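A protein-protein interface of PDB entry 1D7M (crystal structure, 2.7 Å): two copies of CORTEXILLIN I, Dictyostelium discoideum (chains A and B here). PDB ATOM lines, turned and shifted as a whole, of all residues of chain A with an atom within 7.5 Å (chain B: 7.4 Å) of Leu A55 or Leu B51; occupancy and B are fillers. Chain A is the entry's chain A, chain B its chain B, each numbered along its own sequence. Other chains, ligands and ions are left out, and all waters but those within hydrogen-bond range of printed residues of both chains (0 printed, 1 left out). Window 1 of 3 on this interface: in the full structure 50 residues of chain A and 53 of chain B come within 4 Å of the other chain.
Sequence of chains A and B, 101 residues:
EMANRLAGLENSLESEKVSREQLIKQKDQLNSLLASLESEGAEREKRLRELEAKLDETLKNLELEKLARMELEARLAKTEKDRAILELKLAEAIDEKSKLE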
ATOM      1  N   ARG A  47     -21.225 -27.835 -17.957  1.00  0.00           N
ATOM      2  CA  ARG A  47     -20.053 -26.988 -17.753  1.00  0.00           C
ATOM      3  C   ARG A  47     -19.627 -26.969 -16.296  1.00  0.00           C
ATOM      4  O   ARG A  47     -18.438 -26.955 -16.015  1.00  0.00           O
ATOM      5  CB  ARG A  47     -20.296 -25.543 -18.213  1.00  0.00           C
ATOM      6  CG  ARG A  47     -18.972 -24.765 -18.405  1.00  0.00           C
ATOM      7  CD  ARG A  47     -19.036 -23.332 -17.858  1.00  0.00           C
ATOM      8  NE  ARG A  47     -18.386 -22.343 -18.723  1.00  0.00           N
ATOM      9  CZ  ARG A  47     -18.748 -21.061 -18.801  1.00  0.00           C
ATOM     10  NH1 ARG A  47     -19.751 -20.607 -18.066  1.00  0.00           N
ATOM     11  NH2 ARG A  47     -18.124 -20.231 -19.629  1.00  0.00           N
ATOM     12  N   LEU A  48     -20.599 -26.968 -15.386  1.00  0.00           N
ATOM     13  CA  LEU A  48     -20.340 -26.952 -13.947  1.00  0.00           C
ATOM     14  C   LEU A  48     -19.647 -28.275 -13.585  1.00  0.00           C
ATOM     15  O   LEU A  48     -18.602 -28.279 -12.945  1.00  0.00           O
ATOM     16  CB  LEU A  48     -21.678 -26.799 -13.215  1.00  0.00           C
ATOM     17  CG  LEU A  48     -21.908 -26.359 -11.769  1.00  0.00           C
ATOM     18  CD1 LEU A  48     -21.575 -24.908 -11.575  1.00  0.00           C
ATOM     19  CD2 LEU A  48     -23.376 -26.571 -11.461  1.00  0.00           C
ATOM     20  N   ARG A  49     -20.219 -29.394 -14.015  1.00  0.00           N
ATOM     21  CA  ARG A  49     -19.616 -30.704 -13.761  1.00  0.00           C
ATOM     22  C   ARG A  49     -18.126 -30.683 -14.200  1.00  0.00           C
ATOM     23  O   ARG A  49     -17.243 -31.141 -13.472  1.00  0.00           O
ATOM     24  CB  ARG A  49     -20.403 -31.763 -14.543  1.00  0.00           C
ATOM     25  CG  ARG A  49     -20.275 -33.199 -14.041  1.00  0.00           C
ATOM     26  CD  ARG A  49     -21.087 -33.498 -12.767  1.00  0.00           C
ATOM     27  NE  ARG A  49     -20.427 -34.555 -12.001  1.00  0.00           N
ATOM     28  CZ  ARG A  49     -20.979 -35.303 -11.046  1.00  0.00           C
ATOM     29  NH1 ARG A  49     -22.249 -35.148 -10.690  1.00  0.00           N
ATOM     30  NH2 ARG A  49     -20.239 -36.225 -10.439  1.00  0.00           N
ATOM     31  N   GLU A  50     -17.858 -30.143 -15.388  1.00  0.00           N
ATOM     32  CA  GLU A  50     -16.489 -30.061 -15.905  1.00  0.00           C
ATOM     33  C   GLU A  50     -15.609 -29.223 -14.997  1.00  0.00           C
ATOM     34  O   GLU A  50     -14.506 -29.638 -14.632  1.00  0.00           O
ATOM     35  CB  GLU A  50     -16.465 -29.448 -17.303  1.00  0.00           C
ATOM     36  CG  GLU A  50     -17.428 -30.094 -18.265  1.00  0.00           C
ATOM     37  CD  GLU A  50     -17.185 -29.681 -19.697  1.00  0.00           C
ATOM     38  OE1 GLU A  50     -17.075 -28.464 -19.954  1.00  0.00           O
ATOM     39  OE2 GLU A  50     -17.111 -30.580 -20.559  1.00  0.00           O
ATOM     40  N   LEU A  51     -16.083 -28.035 -14.641  1.00  0.00           N
ATOM     41  CA  LEU A  51     -15.295 -27.181 -13.765  1.00  0.00           C
ATOM     42  C   LEU A  51     -14.961 -27.864 -12.460  1.00  0.00           C
ATOM     43  O   LEU A  51     -13.838 -27.734 -11.974  1.00  0.00           O
ATOM     44  CB  LEU A  51     -16.002 -25.854 -13.480  1.00  0.00           C
ATOM     45  CG  LEU A  51     -15.820 -24.860 -14.628  1.00  0.00           C
ATOM     46  CD1 LEU A  51     -15.751 -23.439 -14.081  1.00  0.00           C
ATOM     47  CD2 LEU A  51     -14.533 -25.199 -15.386  1.00  0.00           C
ATOM     48  N   GLU A  52     -15.917 -28.591 -11.891  1.00  0.00           N
ATOM     49  CA  GLU A  52     -15.666 -29.278 -10.633  1.00  0.00           C
ATOM     50  C   GLU A  52     -14.576 -30.325 -10.812  1.00  0.00           C
ATOM     51  O   GLU A  52     -13.631 -30.380 -10.029  1.00  0.00           O
ATOM     52  CB  GLU A  52     -16.974 -29.873 -10.074  1.00  0.00           C
ATOM     53  CG  GLU A  52     -17.878 -28.781  -9.451  1.00  0.00           C
ATOM     54  CD  GLU A  52     -19.305 -29.232  -9.128  1.00  0.00           C
ATOM     55  OE1 GLU A  52     -19.797 -30.177  -9.780  1.00  0.00           O
ATOM     56  OE2 GLU A  52     -19.943 -28.624  -8.239  1.00  0.00           O
ATOM     57  N   ALA A  53     -14.666 -31.140 -11.853  1.00  0.00           N
ATOM     58  CA  ALA A  53     -13.615 -32.118 -12.060  1.00  0.00           C
ATOM     59  C   ALA A  53     -12.270 -31.384 -12.135  1.00  0.00           C
ATOM     60  O   ALA A  53     -11.332 -31.727 -11.421  1.00  0.00           O
ATOM     61  CB  ALA A  53     -13.869 -32.891 -13.333  1.00  0.00           C
ATOM     62  N   LYS A  54     -12.182 -30.360 -12.973  1.00  0.00           N
ATOM     63  CA  LYS A  54     -10.928 -29.618 -13.111  1.00  0.00           C
ATOM     64  C   LYS A  54     -10.398 -29.058 -11.793  1.00  0.00           C
ATOM     65  O   LYS A  54      -9.200 -29.137 -11.517  1.00  0.00           O
ATOM     66  CB  LYS A  54     -11.084 -28.473 -14.114  1.00  0.00           C
ATOM     67  CG  LYS A  54      -9.744 -27.963 -14.636  1.00  0.00           C
ATOM     68  CD  LYS A  54      -9.036 -29.042 -15.477  1.00  0.00           C
ATOM     69  CE  LYS A  54      -7.527 -28.795 -15.664  1.00  0.00           C
ATOM     70  NZ  LYS A  54      -6.670 -29.267 -14.526  1.00  0.00           N
ATOM     71  N   LEU A  55     -11.291 -28.482 -10.990  1.00  0.00           N
ATOM     72  CA  LEU A  55     -10.910 -27.909  -9.701  1.00  0.00           C
ATOM     73  C   LEU A  55     -10.399 -28.963  -8.743  1.00  0.00           C
ATOM     74  O   LEU A  55      -9.529 -28.693  -7.924  1.00  0.00           O
ATOM     75  CB  LEU A  55     -12.100 -27.194  -9.050  1.00  0.00           C
ATOM     76  CG  LEU A  55     -11.795 -26.519  -7.707  1.00  0.00           C
ATOM     77  CD1 LEU A  55     -10.569 -25.646  -7.862  1.00  0.00           C
ATOM     78  CD2 LEU A  55     -12.959 -25.659  -7.257  1.00  0.00           C
ATOM     79  N   ASP A  56     -10.953 -30.162  -8.824  1.00  0.00           N
ATOM     80  CA  ASP A  56     -10.512 -31.205  -7.918  1.00  0.00           C
ATOM     81  C   ASP A  56      -9.081 -31.564  -8.277  1.00  0.00           C
ATOM     82  O   ASP A  56      -8.192 -31.597  -7.427  1.00  0.00           O
ATOM     83  CB  ASP A  56     -11.395 -32.443  -8.039  1.00  0.00           C
ATOM     84  CG  ASP A  56     -11.081 -33.476  -6.984  1.00  0.00           C
ATOM     85  OD1 ASP A  56     -11.775 -33.472  -5.949  1.00  0.00           O
ATOM     86  OD2 ASP A  56     -10.134 -34.267  -7.183  1.00  0.00           O
ATOM     87  N   GLU A  57      -8.861 -31.819  -9.558  1.00  0.00           N
ATOM     88  CA  GLU A  57      -7.551 -32.172 -10.062  1.00  0.00           C
ATOM     89  C   GLU A  57      -6.529 -31.122  -9.653  1.00  0.00           C
ATOM     90  O   GLU A  57      -5.569 -31.400  -8.922  1.00  0.00           O
ATOM     91  CB  GLU A  57      -7.613 -32.236 -11.583  1.00  0.00           C
ATOM     92  CG  GLU A  57      -6.572 -33.115 -12.233  1.00  0.00           C
ATOM     93  CD  GLU A  57      -6.704 -33.148 -13.753  1.00  0.00           C
ATOM     94  OE1 GLU A  57      -6.288 -32.172 -14.419  1.00  0.00           O
ATOM     95  OE2 GLU A  57      -7.233 -34.150 -14.277  1.00  0.00           O
ATOM     96  N   THR A  58      -6.739 -29.911 -10.142  1.00  0.00           N
ATOM     97  CA  THR A  58      -5.821 -28.836  -9.845  1.00  0.00           C
ATOM     98  C   THR A  58      -5.574 -28.790  -8.345  1.00  0.00           C
ATOM     99  O   THR A  58      -4.426 -28.703  -7.924  1.00  0.00           O
ATOM    100  CB  THR A  58      -6.355 -27.494 -10.400  1.00  0.00           C
ATOM    101  OG1 THR A  58      -6.590 -27.649 -11.808  1.00  0.00           O
ATOM    102  CG2 THR A  58      -5.337 -26.338 -10.179  1.00  0.00           C
ATOM    103  N   LEU A  59      -6.620 -28.890  -7.531  1.00  0.00           N
ATOM    104  CA  LEU A  59      -6.415 -28.861  -6.083  1.00  0.00           C
ATOM    105  C   LEU A  59      -5.442 -29.944  -5.620  1.00  0.00           C
ATOM    106  O   LEU A  59      -4.549 -29.672  -4.810  1.00  0.00           O
ATOM    107  CB  LEU A  59      -7.757 -29.016  -5.366  1.00  0.00           C
ATOM    108  CG  LEU A  59      -8.267 -27.803  -4.584  1.00  0.00           C
ATOM    109  CD1 LEU A  59      -7.570 -26.518  -5.016  1.00  0.00           C
ATOM    110  CD2 LEU A  59      -9.764 -27.720  -4.787  1.00  0.00           C
ATOM    111  N   LYS A  60      -5.618 -31.170  -6.127  1.00  0.00           N
ATOM    112  CA  LYS A  60      -4.714 -32.266  -5.757  1.00  0.00           C
ATOM    113  C   LYS A  60      -3.312 -31.778  -6.066  1.00  0.00           C
ATOM    114  O   LYS A  60      -2.469 -31.692  -5.189  1.00  0.00           O
ATOM    115  CB  LYS A  60      -4.984 -33.537  -6.581  1.00  0.00           C
ATOM    116  CG  LYS A  60      -6.325 -34.224  -6.314  1.00  0.00           C
ATOM    117  CD  LYS A  60      -6.307 -35.178  -5.111  1.00  0.00           C
ATOM    118  CE  LYS A  60      -7.731 -35.684  -4.726  1.00  0.00           C
ATOM    119  NZ  LYS A  60      -8.333 -36.852  -5.470  1.00  0.00           N
ATOM    120  N   ASN A  61      -3.086 -31.448  -7.327  1.00  0.00           N
ATOM    121  CA  ASN A  61      -1.799 -30.962  -7.787  1.00  0.00           C
ATOM    122  C   ASN A  61      -1.198 -29.867  -6.912  1.00  0.00           C
ATOM    123  O   ASN A  61      -0.019 -29.921  -6.552  1.00  0.00           O
ATOM    124  CB  ASN A  61      -1.961 -30.477  -9.220  1.00  0.00           C
ATOM    125  CG  ASN A  61      -2.403 -31.596 -10.158  1.00  0.00           C
ATOM    126  OD1 ASN A  61      -1.637 -32.513 -10.452  1.00  0.00           O
ATOM    127  ND2 ASN A  61      -3.647 -31.529 -10.622  1.00  0.00           N
ATOM    128  N   GLU B  45     -25.866 -20.341 -11.645  1.00  0.00           N
ATOM    129  CA  GLU B  45     -24.922 -19.446 -12.294  1.00  0.00           C
ATOM    130  C   GLU B  45     -24.040 -18.797 -11.260  1.00  0.00           C
ATOM    131  O   GLU B  45     -22.882 -18.497 -11.530  1.00  0.00           O
ATOM    132  CB  GLU B  45     -25.632 -18.364 -13.099  1.00  0.00           C
ATOM    133  CG  GLU B  45     -26.048 -18.809 -14.487  1.00  0.00           C
ATOM    134  CD  GLU B  45     -24.873 -19.208 -15.376  1.00  0.00           C
ATOM    135  OE1 GLU B  45     -23.825 -18.526 -15.354  1.00  0.00           O
ATOM    136  OE2 GLU B  45     -25.006 -20.199 -16.119  1.00  0.00           O
ATOM    137  N   LYS B  46     -24.582 -18.578 -10.072  1.00  0.00           N
ATOM    138  CA  LYS B  46     -23.787 -17.968  -9.020  1.00  0.00           C
ATOM    139  C   LYS B  46     -22.712 -18.973  -8.623  1.00  0.00           C
ATOM    140  O   LYS B  46     -21.529 -18.649  -8.535  1.00  0.00           O
ATOM    141  CB  LYS B  46     -24.680 -17.621  -7.827  1.00  0.00           C
ATOM    142  CG  LYS B  46     -23.925 -17.365  -6.540  1.00  0.00           C
ATOM    143  CD  LYS B  46     -24.839 -17.641  -5.346  1.00  0.00           C
ATOM    144  CE  LYS B  46     -24.147 -17.443  -3.991  1.00  0.00           C
ATOM    145  NZ  LYS B  46     -25.041 -17.767  -2.825  1.00  0.00           N
ATOM    146  N   ARG B  47     -23.155 -20.202  -8.408  1.00  0.00           N
ATOM    147  CA  ARG B  47     -22.287 -21.305  -8.049  1.00  0.00           C
ATOM    148  C   ARG B  47     -21.182 -21.527  -9.099  1.00  0.00           C
ATOM    149  O   ARG B  47     -20.032 -21.805  -8.755  1.00  0.00           O
ATOM    150  CB  ARG B  47     -23.160 -22.540  -7.921  1.00  0.00           C
ATOM    151  CG  ARG B  47     -22.479 -23.801  -8.277  1.00  0.00           C
ATOM    152  CD  ARG B  47     -21.573 -24.202  -7.169  1.00  0.00           C
ATOM    153  NE  ARG B  47     -21.651 -25.639  -6.989  1.00  0.00           N
ATOM    154  CZ  ARG B  47     -20.860 -26.326  -6.184  1.00  0.00           C
ATOM    155  NH1 ARG B  47     -21.006 -27.639  -6.082  1.00  0.00           N
ATOM    156  NH2 ARG B  47     -19.924 -25.699  -5.484  1.00  0.00           N
ATOM    157  N   LEU B  48     -21.553 -21.411 -10.371  1.00  0.00           N
ATOM    158  CA  LEU B  48     -20.611 -21.585 -11.477  1.00  0.00           C
ATOM    159  C   LEU B  48     -19.594 -20.467 -11.410  1.00  0.00           C
ATOM    160  O   LEU B  48     -18.397 -20.713 -11.461  1.00  0.00           O
ATOM    161  CB  LEU B  48     -21.328 -21.521 -12.830  1.00  0.00           C
ATOM    162  CG  LEU B  48     -20.473 -22.019 -14.004  1.00  0.00           C
ATOM    163  CD1 LEU B  48     -20.499 -23.542 -14.001  1.00  0.00           C
ATOM    164  CD2 LEU B  48     -20.991 -21.492 -15.345  1.00  0.00           C
ATOM    165  N   ARG B  49     -20.064 -19.232 -11.317  1.00  0.00           N
ATOM    166  CA  ARG B  49     -19.136 -18.118 -11.220  1.00  0.00           C
ATOM    167  C   ARG B  49     -18.107 -18.352 -10.101  1.00  0.00           C
ATOM    168  O   ARG B  49     -16.910 -18.133 -10.289  1.00  0.00           O
ATOM    169  CB  ARG B  49     -19.916 -16.819 -10.999  1.00  0.00           C
ATOM    170  CG  ARG B  49     -20.315 -16.162 -12.308  1.00  0.00           C
ATOM    171  CD  ARG B  49     -20.962 -14.799 -12.105  1.00  0.00           C
ATOM    172  NE  ARG B  49     -22.329 -14.907 -11.603  1.00  0.00           N
ATOM    173  CZ  ARG B  49     -22.709 -14.706 -10.343  1.00  0.00           C
ATOM    174  NH1 ARG B  49     -21.825 -14.368  -9.415  1.00  0.00           N
ATOM    175  NH2 ARG B  49     -23.984 -14.861 -10.018  1.00  0.00           N
ATOM    176  N   GLU B  50     -18.570 -18.820  -8.948  1.00  0.00           N
ATOM    177  CA  GLU B  50     -17.668 -19.097  -7.832  1.00  0.00           C
ATOM    178  C   GLU B  50     -16.650 -20.170  -8.189  1.00  0.00           C
ATOM    179  O   GLU B  50     -15.458 -20.002  -7.955  1.00  0.00           O
ATOM    180  CB  GLU B  50     -18.466 -19.522  -6.606  1.00  0.00           C
ATOM    181  CG  GLU B  50     -19.333 -18.396  -6.098  1.00  0.00           C
ATOM    182  CD  GLU B  50     -20.258 -18.825  -4.990  1.00  0.00           C
ATOM    183  OE1 GLU B  50     -20.513 -20.043  -4.893  1.00  0.00           O
ATOM    184  OE2 GLU B  50     -20.736 -17.950  -4.236  1.00  0.00           O
ATOM    185  N   LEU B  51     -17.119 -21.272  -8.758  1.00  0.00           N
ATOM    186  CA  LEU B  51     -16.223 -22.340  -9.165  1.00  0.00           C
ATOM    187  C   LEU B  51     -15.140 -21.841 -10.094  1.00  0.00           C
ATOM    188  O   LEU B  51     -13.983 -22.221  -9.959  1.00  0.00           O
ATOM    189  CB  LEU B  51     -17.002 -23.435  -9.867  1.00  0.00           C
ATOM    190  CG  LEU B  51     -17.146 -24.615  -8.930  1.00  0.00           C
ATOM    191  CD1 LEU B  51     -15.801 -25.272  -8.918  1.00  0.00           C
ATOM    192  CD2 LEU B  51     -17.578 -24.189  -7.511  1.00  0.00           C
ATOM    193  N   GLU B  52     -15.531 -21.011 -11.055  1.00  0.00           N
ATOM    194  CA  GLU B  52     -14.596 -20.447 -12.016  1.00  0.00           C
ATOM    195  C   GLU B  52     -13.522 -19.647 -11.297  1.00  0.00           C
ATOM    196  O   GLU B  52     -12.324 -19.851 -11.506  1.00  0.00           O
ATOM    197  CB  GLU B  52     -15.342 -19.568 -13.026  1.00  0.00           C
ATOM    198  CG  GLU B  52     -16.020 -20.363 -14.148  1.00  0.00           C
ATOM    199  CD  GLU B  52     -16.647 -19.496 -15.230  1.00  0.00           C
ATOM    200  OE1 GLU B  52     -17.097 -20.054 -16.258  1.00  0.00           O
ATOM    201  OE2 GLU B  52     -16.693 -18.262 -15.053  1.00  0.00           O
ATOM    202  N   ALA B  53     -13.936 -18.725 -10.444  1.00  0.00           N
ATOM    203  CA  ALA B  53     -12.947 -17.957  -9.712  1.00  0.00           C
ATOM    204  C   ALA B  53     -11.997 -18.932  -9.003  1.00  0.00           C
ATOM    205  O   ALA B  53     -10.783 -18.848  -9.177  1.00  0.00           O
ATOM    206  CB  ALA B  53     -13.623 -17.031  -8.705  1.00  0.00           C
ATOM    207  N   LYS B  54     -12.535 -19.868  -8.225  1.00  0.00           N
ATOM    208  CA  LYS B  54     -11.681 -20.825  -7.509  1.00  0.00           C
ATOM    209  C   LYS B  54     -10.696 -21.562  -8.408  1.00  0.00           C
ATOM    210  O   LYS B  54      -9.538 -21.745  -8.042  1.00  0.00           O
ATOM    211  CB  LYS B  54     -12.529 -21.847  -6.749  1.00  0.00           C
ATOM    212  CG  LYS B  54     -12.430 -21.742  -5.231  1.00  0.00           C
ATOM    213  CD  LYS B  54     -10.984 -21.891  -4.752  1.00  0.00           C
ATOM    214  CE  LYS B  54     -10.844 -21.974  -3.213  1.00  0.00           C
ATOM    215  NZ  LYS B  54     -10.935 -23.359  -2.623  1.00  0.00           N
ATOM    216  N   LEU B  55     -11.138 -22.001  -9.576  1.00  0.00           N
ATOM    217  CA  LEU B  55     -10.211 -22.706 -10.449  1.00  0.00           C
ATOM    218  C   LEU B  55      -9.124 -21.757 -10.943  1.00  0.00           C
ATOM    219  O   LEU B  55      -7.994 -22.179 -11.171  1.00  0.00           O
ATOM    220  CB  LEU B  55     -10.938 -23.309 -11.649  1.00  0.00           C
ATOM    221  CG  LEU B  55     -10.135 -24.331 -12.458  1.00  0.00           C
ATOM    222  CD1 LEU B  55      -9.957 -25.573 -11.611  1.00  0.00           C
ATOM    223  CD2 LEU B  55     -10.852 -24.707 -13.750  1.00  0.00           C
ATOM    224  N   ASP B  56      -9.457 -20.476 -11.121  1.00  0.00           N
ATOM    225  CA  ASP B  56      -8.454 -19.527 -11.598  1.00  0.00           C
ATOM    226  C   ASP B  56      -7.421 -19.374 -10.516  1.00  0.00           C
ATOM    227  O   ASP B  56      -6.219 -19.516 -10.760  1.00  0.00           O
ATOM    228  CB  ASP B  56      -9.038 -18.136 -11.881  1.00  0.00           C
ATOM    229  CG  ASP B  56      -9.920 -18.099 -13.112  1.00  0.00           C
ATOM    230  OD1 ASP B  56      -9.497 -18.628 -14.162  1.00  0.00           O
ATOM    231  OD2 ASP B  56     -11.025 -17.520 -13.017  1.00  0.00           O
ATOM    232  N   GLU B  57      -7.898 -19.082  -9.314  1.00  0.00           N
ATOM    233  CA  GLU B  57      -6.995 -18.885  -8.198  1.00  0.00           C
ATOM    234  C   GLU B  57      -6.093 -20.082  -7.991  1.00  0.00           C
ATOM    235  O   GLU B  57      -4.870 -19.978  -8.061  1.00  0.00           O
ATOM    236  CB  GLU B  57      -7.756 -18.596  -6.903  1.00  0.00           C
ATOM    237  CG  GLU B  57      -6.910 -17.685  -6.042  1.00  0.00           C
ATOM    238  CD  GLU B  57      -7.079 -17.882  -4.556  1.00  0.00           C
ATOM    239  OE1 GLU B  57      -6.218 -17.364  -3.814  1.00  0.00           O
ATOM    240  OE2 GLU B  57      -8.060 -18.537  -4.140  1.00  0.00           O
ATOM    241  N   THR B  58      -6.708 -21.225  -7.730  1.00  0.00           N
ATOM    242  CA  THR B  58      -5.948 -22.437  -7.529  1.00  0.00           C
ATOM    243  C   THR B  58      -4.927 -22.581  -8.647  1.00  0.00           C
ATOM    244  O   THR B  58      -3.761 -22.833  -8.378  1.00  0.00           O
ATOM    245  CB  THR B  58      -6.900 -23.641  -7.442  1.00  0.00           C
ATOM    246  OG1 THR B  58      -7.622 -23.548  -6.208  1.00  0.00           O
ATOM    247  CG2 THR B  58      -6.140 -24.990  -7.533  1.00  0.00           C
ATOM    248  N   LEU B  59      -5.344 -22.390  -9.893  1.00  0.00           N
ATOM    249  CA  LEU B  59      -4.414 -22.492 -11.013  1.00  0.00           C
ATOM    250  C   LEU B  59      -3.186 -21.595 -10.820  1.00  0.00           C
ATOM    251  O   LEU B  59      -2.045 -22.022 -11.015  1.00  0.00           O
ATOM    252  CB  LEU B  59      -5.119 -22.112 -12.313  1.00  0.00           C
ATOM    253  CG  LEU B  59      -5.352 -23.218 -13.346  1.00  0.00           C
ATOM    254  CD1 LEU B  59      -4.141 -24.113 -13.356  1.00  0.00           C
ATOM    255  CD2 LEU B  59      -6.587 -24.032 -13.024  1.00  0.00           C
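The backbone carbonyl oxygen of Lys A54 lies within hydrogen-bond range of the side-chain hydroxyl of Thr A58, 3.0 Å away.
The side-chain carboxylate (OE1) of Glu A57 is in salt-bridge range of the side-chain amino group (NZ) of Lys A54 (2.9 Å).
O of Lys B54 is in hydrogen-bond range of OG1 of Thr B58.
Among the printed residues, merely in contact across the chains: Leu A48 with Leu B48 (3.0 Å), Thr A58 with Thr B58 (3.1 Å), Leu A51 with Glu B52 (3.1 Å), Arg A47 with Leu B48 (3.1 Å), Leu A55 with Leu B55 (3.2 Å), Leu A59 with Thr B58 (3.2 Å), Leu A55 with Leu B51 (3.3 Å), Lys A54 with Leu B55 (3.5 Å), Leu A48 with Arg B47 (3.6 Å), Thr A58 with Leu B59 (3.8 Å), Leu A55 with Lys B54 (3.9 Å), Thr A58 with Leu B55 (3.96 Å) and Leu A55 with Thr B58 (3.98 Å).
Printed residues of chain B within 4 Å of Lys A54: Leu B55.
Of chain B, only Leu B51, Lys B54, Leu B55 and Thr B58 come within 4 Å of Leu A55.
Printed residues of chain B within 4 Å of Thr A58: Leu B55 (3.96 Å), Thr B58 (3.1 Å) and Leu B59 (3.8 Å).
Leu B51 touches just one residue of chain A: Leu A55 (3.3 Å).
The nearest printed residue of chain B that does not touch Leu A55 is Asp B56 (6.2 Å).
The side-chain carboxylate (OE2) of Glu A52 is in salt-bridge range of the guanidinium group (NH1) of Arg B47, 2.6 Å away.
The side-chain carboxylate (OE1) of Glu B52 is in salt-bridge range of the guanidinium group (NH1) of Arg A47, at 3.3 Å.
Arg A47 touches Glu B52, and with the chains exchanged Glu A52 touches Arg B47.
Lys A54 touches Leu B55, and with the chains exchanged Leu A55 touches Lys B54.
Leu A55 touches Thr B58, and with the chains exchanged Thr A58 touches Leu B55.
Thr A58 touches Leu B59, and with the chains exchanged Leu A59 touches Thr B58.
13 positions are printed for both chains.
Of the 15 pairs that touch across the chains among the printed residues, 13 have their exchanged pair printed and touching as well.
Hydrophobic or aromatic side chains of chain B within 4 Å of the printed part of chain A: Leu B48, Leu B51, Leu B55 and Leu B59.
Along chain B the printed residues that touch a printed residue of chain A span positions 47 to 59.
Hydrophobic or aromatic side chains of chain A within 4 Å of the printed part of chain B: Leu A48, Leu A51, Leu A55 and Leu A59.
Among the printed residues, Asp or Glu carboxylates within 4 Å of a Lys or Arg side-chain nitrogen of the other chain: Arg A47 with Glu B52 and Glu A52 with Arg B47.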
